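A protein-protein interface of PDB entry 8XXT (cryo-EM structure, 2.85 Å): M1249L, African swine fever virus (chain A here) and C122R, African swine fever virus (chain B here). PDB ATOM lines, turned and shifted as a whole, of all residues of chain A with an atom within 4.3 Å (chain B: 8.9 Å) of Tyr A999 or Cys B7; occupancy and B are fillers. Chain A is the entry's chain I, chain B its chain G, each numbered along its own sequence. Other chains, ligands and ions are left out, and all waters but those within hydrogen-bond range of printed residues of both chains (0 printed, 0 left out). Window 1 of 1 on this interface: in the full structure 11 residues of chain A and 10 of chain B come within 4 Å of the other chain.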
ATOM      1  N   ARG A 995      -1.351 -16.058  18.785  1.00  0.00           N
ATOM      2  CA  ARG A 995      -2.388 -15.572  19.687  1.00  0.00           C
ATOM      3  C   ARG A 995      -1.791 -15.068  20.992  1.00  0.00           C
ATOM      4  O   ARG A 995      -2.222 -14.039  21.523  1.00  0.00           O
ATOM      5  CB  ARG A 995      -3.404 -16.676  19.967  1.00  0.00           C
ATOM      6  CG  ARG A 995      -4.705 -16.171  20.550  1.00  0.00           C
ATOM      7  CD  ARG A 995      -5.746 -17.270  20.602  1.00  0.00           C
ATOM      8  NE  ARG A 995      -5.764 -18.077  19.390  1.00  0.00           N
ATOM      9  CZ  ARG A 995      -6.218 -17.660  18.215  1.00  0.00           C
ATOM     10  NH1 ARG A 995      -6.691 -16.437  18.049  1.00  0.00           N
ATOM     11  NH2 ARG A 995      -6.200 -18.495  17.182  1.00  0.00           N
ATOM     12  N   ILE A 996      -0.798 -15.783  21.524  1.00  0.00           N
ATOM     13  CA  ILE A 996      -0.179 -15.389  22.787  1.00  0.00           C
ATOM     14  C   ILE A 996       0.432 -14.002  22.667  1.00  0.00           C
ATOM     15  O   ILE A 996       0.277 -13.156  23.556  1.00  0.00           O
ATOM     16  CB  ILE A 996       0.870 -16.433  23.211  1.00  0.00           C
ATOM     17  CG1 ILE A 996       0.205 -17.601  23.927  1.00  0.00           C
ATOM     18  CG2 ILE A 996       1.922 -15.811  24.105  1.00  0.00           C
ATOM     19  CD1 ILE A 996       1.138 -18.752  24.157  1.00  0.00           C
ATOM     20  N   PHE A 997       1.134 -13.747  21.564  1.00  0.00           N
ATOM     21  CA  PHE A 997       1.736 -12.437  21.353  1.00  0.00           C
ATOM     22  C   PHE A 997       0.669 -11.353  21.297  1.00  0.00           C
ATOM     23  O   PHE A 997       0.805 -10.299  21.928  1.00  0.00           O
ATOM     24  CB  PHE A 997       2.560 -12.450  20.070  1.00  0.00           C
ATOM     25  CG  PHE A 997       3.296 -11.175  19.812  1.00  0.00           C
ATOM     26  CD1 PHE A 997       4.400 -10.835  20.571  1.00  0.00           C
ATOM     27  CD2 PHE A 997       2.884 -10.313  18.814  1.00  0.00           C
ATOM     28  CE1 PHE A 997       5.080  -9.664  20.338  1.00  0.00           C
ATOM     29  CE2 PHE A 997       3.560  -9.138  18.579  1.00  0.00           C
ATOM     30  CZ  PHE A 997       4.660  -8.815  19.339  1.00  0.00           C
ATOM     31  N   LEU A 998      -0.410 -11.601  20.554  1.00  0.00           N
ATOM     32  CA  LEU A 998      -1.482 -10.616  20.458  1.00  0.00           C
ATOM     33  C   LEU A 998      -2.230 -10.476  21.775  1.00  0.00           C
ATOM     34  O   LEU A 998      -2.614  -9.368  22.163  1.00  0.00           O
ATOM     35  CB  LEU A 998      -2.444 -11.002  19.338  1.00  0.00           C
ATOM     36  CG  LEU A 998      -1.852 -10.994  17.934  1.00  0.00           C
ATOM     37  CD1 LEU A 998      -2.859 -11.539  16.950  1.00  0.00           C
ATOM     38  CD2 LEU A 998      -1.433  -9.592  17.551  1.00  0.00           C
ATOM     39  N   TYR A 999      -2.453 -11.590  22.474  1.00  0.00           N
ATOM     40  CA  TYR A 999      -3.206 -11.547  23.723  1.00  0.00           C
ATOM     41  C   TYR A 999      -2.492 -10.702  24.768  1.00  0.00           C
ATOM     42  O   TYR A 999      -3.103  -9.837  25.406  1.00  0.00           O
ATOM     43  CB  TYR A 999      -3.435 -12.969  24.239  1.00  0.00           C
ATOM     44  CG  TYR A 999      -3.929 -13.046  25.663  1.00  0.00           C
ATOM     45  CD1 TYR A 999      -5.183 -12.567  26.009  1.00  0.00           C
ATOM     46  CD2 TYR A 999      -3.148 -13.612  26.658  1.00  0.00           C
ATOM     47  CE1 TYR A 999      -5.642 -12.641  27.308  1.00  0.00           C
ATOM     48  CE2 TYR A 999      -3.598 -13.691  27.959  1.00  0.00           C
ATOM     49  CZ  TYR A 999      -4.847 -13.204  28.278  1.00  0.00           C
ATOM     50  OH  TYR A 999      -5.302 -13.280  29.573  1.00  0.00           O
ATOM     51  N   ASN A1000      -1.192 -10.933  24.953  1.00  0.00           N
ATOM     52  CA  ASN A1000      -0.452 -10.187  25.963  1.00  0.00           C
ATOM     53  C   ASN A1000      -0.125  -8.773  25.509  1.00  0.00           C
ATOM     54  O   ASN A1000       0.001  -7.875  26.348  1.00  0.00           O
ATOM     55  CB  ASN A1000       0.831 -10.925  26.329  1.00  0.00           C
ATOM     56  CG  ASN A1000       0.570 -12.214  27.072  1.00  0.00           C
ATOM     57  OD1 ASN A1000      -0.455 -12.368  27.733  1.00  0.00           O
ATOM     58  ND2 ASN A1000       1.501 -13.152  26.969  1.00  0.00           N
ATOM     59  N   TYR A1001       0.029  -8.555  24.202  1.00  0.00           N
ATOM     60  CA  TYR A1001       0.254  -7.200  23.712  1.00  0.00           C
ATOM     61  C   TYR A1001      -0.936  -6.309  24.023  1.00  0.00           C
ATOM     62  O   TYR A1001      -0.767  -5.144  24.400  1.00  0.00           O
ATOM     63  CB  TYR A1001       0.527  -7.215  22.212  1.00  0.00           C
ATOM     64  CG  TYR A1001       0.669  -5.840  21.609  1.00  0.00           C
ATOM     65  CD1 TYR A1001       1.588  -4.934  22.112  1.00  0.00           C
ATOM     66  CD2 TYR A1001      -0.117  -5.447  20.535  1.00  0.00           C
ATOM     67  CE1 TYR A1001       1.724  -3.677  21.563  1.00  0.00           C
ATOM     68  CE2 TYR A1001       0.011  -4.191  19.980  1.00  0.00           C
ATOM     69  CZ  TYR A1001       0.934  -3.310  20.498  1.00  0.00           C
ATOM     70  OH  TYR A1001       1.066  -2.058  19.950  1.00  0.00           O
ATOM     71  N   ASN A1002      -2.151  -6.839  23.868  1.00  0.00           N
ATOM     72  CA  ASN A1002      -3.342  -6.078  24.225  1.00  0.00           C
ATOM     73  C   ASN A1002      -3.387  -5.782  25.717  1.00  0.00           C
ATOM     74  O   ASN A1002      -3.922  -4.744  26.124  1.00  0.00           O
ATOM     75  CB  ASN A1002      -4.596  -6.832  23.793  1.00  0.00           C
ATOM     76  CG  ASN A1002      -4.939  -6.592  22.345  1.00  0.00           C
ATOM     77  OD1 ASN A1002      -5.855  -5.835  22.028  1.00  0.00           O
ATOM     78  ND2 ASN A1002      -4.195  -7.229  21.450  1.00  0.00           N
ATOM     79  N   CYS A1003      -2.840  -6.676  26.544  1.00  0.00           N
ATOM     80  CA  CYS A1003      -2.699  -6.368  27.961  1.00  0.00           C
ATOM     81  C   CYS A1003      -1.789  -5.164  28.163  1.00  0.00           C
ATOM     82  O   CYS A1003      -2.094  -4.270  28.961  1.00  0.00           O
ATOM     83  CB  CYS A1003      -2.156  -7.583  28.714  1.00  0.00           C
ATOM     84  SG  CYS A1003      -3.208  -9.049  28.636  1.00  0.00           S
ATOM     85  N   ILE B   3     -16.689 -12.137  19.705  1.00  0.00           N
ATOM     86  CA  ILE B   3     -15.329 -12.653  19.778  1.00  0.00           C
ATOM     87  C   ILE B   3     -14.358 -11.491  19.627  1.00  0.00           C
ATOM     88  O   ILE B   3     -14.601 -10.556  18.855  1.00  0.00           O
ATOM     89  CB  ILE B   3     -15.080 -13.757  18.728  1.00  0.00           C
ATOM     90  CG1 ILE B   3     -14.227 -14.871  19.335  1.00  0.00           C
ATOM     91  CG2 ILE B   3     -14.441 -13.205  17.462  1.00  0.00           C
ATOM     92  CD1 ILE B   3     -14.962 -15.736  20.327  1.00  0.00           C
ATOM     93  N   CYS B   4     -13.284 -11.528  20.411  1.00  0.00           N
ATOM     94  CA  CYS B   4     -12.304 -10.452  20.394  1.00  0.00           C
ATOM     95  C   CYS B   4     -11.585 -10.428  19.054  1.00  0.00           C
ATOM     96  O   CYS B   4     -11.154 -11.468  18.550  1.00  0.00           O
ATOM     97  CB  CYS B   4     -11.307 -10.630  21.537  1.00  0.00           C
ATOM     98  SG  CYS B   4     -10.056  -9.338  21.658  1.00  0.00           S
ATOM     99  N   LYS B   5     -11.462  -9.237  18.469  1.00  0.00           N
ATOM    100  CA  LYS B   5     -10.816  -9.129  17.168  1.00  0.00           C
ATOM    101  C   LYS B   5      -9.326  -9.436  17.252  1.00  0.00           C
ATOM    102  O   LYS B   5      -8.716  -9.815  16.247  1.00  0.00           O
ATOM    103  CB  LYS B   5     -11.045  -7.737  16.581  1.00  0.00           C
ATOM    104  CG  LYS B   5     -11.640  -7.747  15.182  1.00  0.00           C
ATOM    105  CD  LYS B   5     -13.034  -8.347  15.172  1.00  0.00           C
ATOM    106  CE  LYS B   5     -13.594  -8.409  13.761  1.00  0.00           C
ATOM    107  NZ  LYS B   5     -14.950  -9.020  13.719  1.00  0.00           N
ATOM    108  N   ALA B   6      -8.728  -9.278  18.431  1.00  0.00           N
ATOM    109  CA  ALA B   6      -7.306  -9.530  18.616  1.00  0.00           C
ATOM    110  C   ALA B   6      -7.014 -10.832  19.343  1.00  0.00           C
ATOM    111  O   ALA B   6      -6.077 -11.541  18.963  1.00  0.00           O
ATOM    112  CB  ALA B   6      -6.662  -8.373  19.386  1.00  0.00           C
ATOM    113  N   CYS B   7      -7.789 -11.168  20.372  1.00  0.00           N
ATOM    114  CA  CYS B   7      -7.562 -12.379  21.144  1.00  0.00           C
ATOM    115  C   CYS B   7      -8.386 -13.565  20.672  1.00  0.00           C
ATOM    116  O   CYS B   7      -8.038 -14.704  21.001  1.00  0.00           O
ATOM    117  CB  CYS B   7      -7.862 -12.121  22.628  1.00  0.00           C
ATOM    118  SG  CYS B   7      -7.558 -13.515  23.733  1.00  0.00           S
ATOM    119  N   SER B   8      -9.443 -13.333  19.894  1.00  0.00           N
ATOM    120  CA  SER B   8     -10.369 -14.383  19.474  1.00  0.00           C
ATOM    121  C   SER B   8     -10.912 -15.134  20.687  1.00  0.00           C
ATOM    122  O   SER B   8     -10.925 -16.364  20.742  1.00  0.00           O
ATOM    123  CB  SER B   8      -9.710 -15.338  18.480  1.00  0.00           C
ATOM    124  OG  SER B   8     -10.685 -16.087  17.781  1.00  0.00           O
ATOM    125  N   SER B   9     -11.358 -14.365  21.674  1.00  0.00           N
ATOM    126  CA  SER B   9     -11.881 -14.899  22.919  1.00  0.00           C
ATOM    127  C   SER B   9     -13.290 -14.377  23.143  1.00  0.00           C
ATOM    128  O   SER B   9     -13.656 -13.306  22.654  1.00  0.00           O
ATOM    129  CB  SER B   9     -10.996 -14.522  24.107  1.00  0.00           C
ATOM    130  OG  SER B   9     -11.773 -14.338  25.278  1.00  0.00           O
ATOM    131  N   CYS B  10     -14.080 -15.153  23.877  1.00  0.00           N
ATOM    132  CA  CYS B  10     -15.444 -14.753  24.184  1.00  0.00           C
ATOM    133  C   CYS B  10     -15.438 -13.602  25.180  1.00  0.00           C
ATOM    134  O   CYS B  10     -14.713 -13.632  26.178  1.00  0.00           O
ATOM    135  CB  CYS B  10     -16.230 -15.938  24.738  1.00  0.00           C
ATOM    136  SG  CYS B  10     -16.628 -17.195  23.508  1.00  0.00           S
ATOM    137  N   MET B  11     -16.254 -12.588  24.910  1.00  0.00           N
ATOM    138  CA  MET B  11     -16.275 -11.355  25.683  1.00  0.00           C
ATOM    139  C   MET B  11     -17.531 -11.305  26.544  1.00  0.00           C
ATOM    140  O   MET B  11     -18.630 -11.596  26.063  1.00  0.00           O
ATOM    141  CB  MET B  11     -16.227 -10.140  24.757  1.00  0.00           C
ATOM    142  CG  MET B  11     -15.604 -10.422  23.405  1.00  0.00           C
ATOM    143  SD  MET B  11     -15.352  -8.939  22.414  1.00  0.00           S
ATOM    144  CE  MET B  11     -14.433  -7.916  23.555  1.00  0.00           C
ATOM    145  N   CYS B  24     -13.199  -8.054  26.808  1.00  0.00           N
ATOM    146  CA  CYS B  24     -12.407  -9.270  26.694  1.00  0.00           C
ATOM    147  C   CYS B  24     -11.460  -9.401  27.880  1.00  0.00           C
ATOM    148  O   CYS B  24     -11.253  -8.465  28.654  1.00  0.00           O
ATOM    149  CB  CYS B  24     -11.620  -9.278  25.382  1.00  0.00           C
ATOM    150  SG  CYS B  24     -10.692 -10.797  25.080  1.00  0.00           S
ATOM    151  N   SER B  25     -10.876 -10.593  28.017  1.00  0.00           N
ATOM    152  CA  SER B  25      -9.866 -10.805  29.046  1.00  0.00           C
ATOM    153  C   SER B  25      -8.601 -10.003  28.777  1.00  0.00           C
ATOM    154  O   SER B  25      -7.807  -9.791  29.700  1.00  0.00           O
ATOM    155  CB  SER B  25      -9.528 -12.290  29.156  1.00  0.00           C
ATOM    156  OG  SER B  25      -9.179 -12.636  30.485  1.00  0.00           O
ATOM    157  N   CYS B  26      -8.399  -9.555  27.541  1.00  0.00           N
ATOM    158  CA  CYS B  26      -7.262  -8.727  27.173  1.00  0.00           C
ATOM    159  C   CYS B  26      -7.511  -7.247  27.436  1.00  0.00           C
ATOM    160  O   CYS B  26      -6.642  -6.420  27.141  1.00  0.00           O
ATOM    161  CB  CYS B  26      -6.913  -8.942  25.699  1.00  0.00           C
ATOM    162  SG  CYS B  26      -8.167  -8.347  24.544  1.00  0.00           S
ATOM    163  N   GLY B  27      -8.676  -6.896  27.974  1.00  0.00           N
ATOM    164  CA  GLY B  27      -8.997  -5.522  28.276  1.00  0.00           C
ATOM    165  C   GLY B  27      -9.616  -4.742  27.141  1.00  0.00           C
ATOM    166  O   GLY B  27     -10.030  -3.596  27.357  1.00  0.00           O
ATOM    167  N   GLU B  28      -9.698  -5.313  25.944  1.00  0.00           N
ATOM    168  CA  GLU B  28     -10.305  -4.609  24.826  1.00  0.00           C
ATOM    169  C   GLU B  28     -11.810  -4.496  25.016  1.00  0.00           C
ATOM    170  O   GLU B  28     -12.446  -5.369  25.613  1.00  0.00           O
ATOM    171  CB  GLU B  28     -10.000  -5.321  23.512  1.00  0.00           C
ATOM    172  CG  GLU B  28     -10.048  -4.409  22.300  1.00  0.00           C
ATOM    173  CD  GLU B  28     -10.655  -5.084  21.087  1.00  0.00           C
ATOM    174  OE1 GLU B  28     -10.351  -6.271  20.855  1.00  0.00           O
ATOM    175  OE2 GLU B  28     -11.436  -4.427  20.368  1.00  0.00           O
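The backbone carbonyl oxygen (O) of Asn A1002 sits close to the backbone carbonyl oxygen (O) of Cys B26.
Of the printed residues of chain A, Cys B7 touches Arg A995 (3.5 Å) and Tyr A999 (3.4 Å).
No residue of chain B comes within 4 Å of Asn A1000.
Of the printed residues of chain B, Arg A995 touches Cys B7 and Ser B8.
Of the printed residues of chain A, Ala B6 touches Leu A998 (3.7 Å) and Asn A1002 (3.4 Å).
Printed residues of chain B within 4 Å of Leu A998: Ala B6 (3.7 Å).
Printed residues of chain B within 4 Å of Asn A1002: Ala B6 and Cys B26.
Gly B27 touches none of the printed residues of chain A.
Ser B9 touches none of the printed residues of chain A.
The nearest residue of chain B that does not touch Tyr A999 is Ser B25 (4.03 Å).
The nearest printed residue of chain B that does not touch Cys A1003 is Ser B25 (4.8 Å).
The side-chain sulfur of Cys B4 sits close to the backbone NH of Ala B6, 3.5 Å away.
N of Cys B7 lies close to SG of Cys B4 (3.2 Å).
The backbone NH of Glu B28 sits close to the side-chain sulfur of Cys B26, 3.7 Å away.
O of Leu A998 sits at hydrogen-bond distance from ND2 of Asn A1002, 2.8 Å away.
The backbone carbonyl oxygen of Tyr A999 lies within hydrogen-bond range of the side-chain sulfur of Cys A1003.
Among the printed residues, pairs that only touch across the chains: Arg A995 with Cys B7, Arg A995 with Ser B8, Leu A998 with Ala B6, Tyr A999 with Cys B7, Tyr A999 with Cys B26, Asn A1002 with Ala B6 and Cys A1003 with Cys B26.
Hydrophobic or aromatic side chains of chain A within 4 Å of the printed part of chain B: Leu A998 and Tyr A999.
Of the 14 printed residues of chain B, 4 touch a printed residue of chain A.
Printed residues of chain B that touch a printed residue of chain A: Ala B6, Cys B7, Ser B8 and Cys B26.
Among the printed residues, no Asp or Glu carboxylate lies within 4 Å of a Lys or Arg side-chain nitrogen of the other chain.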
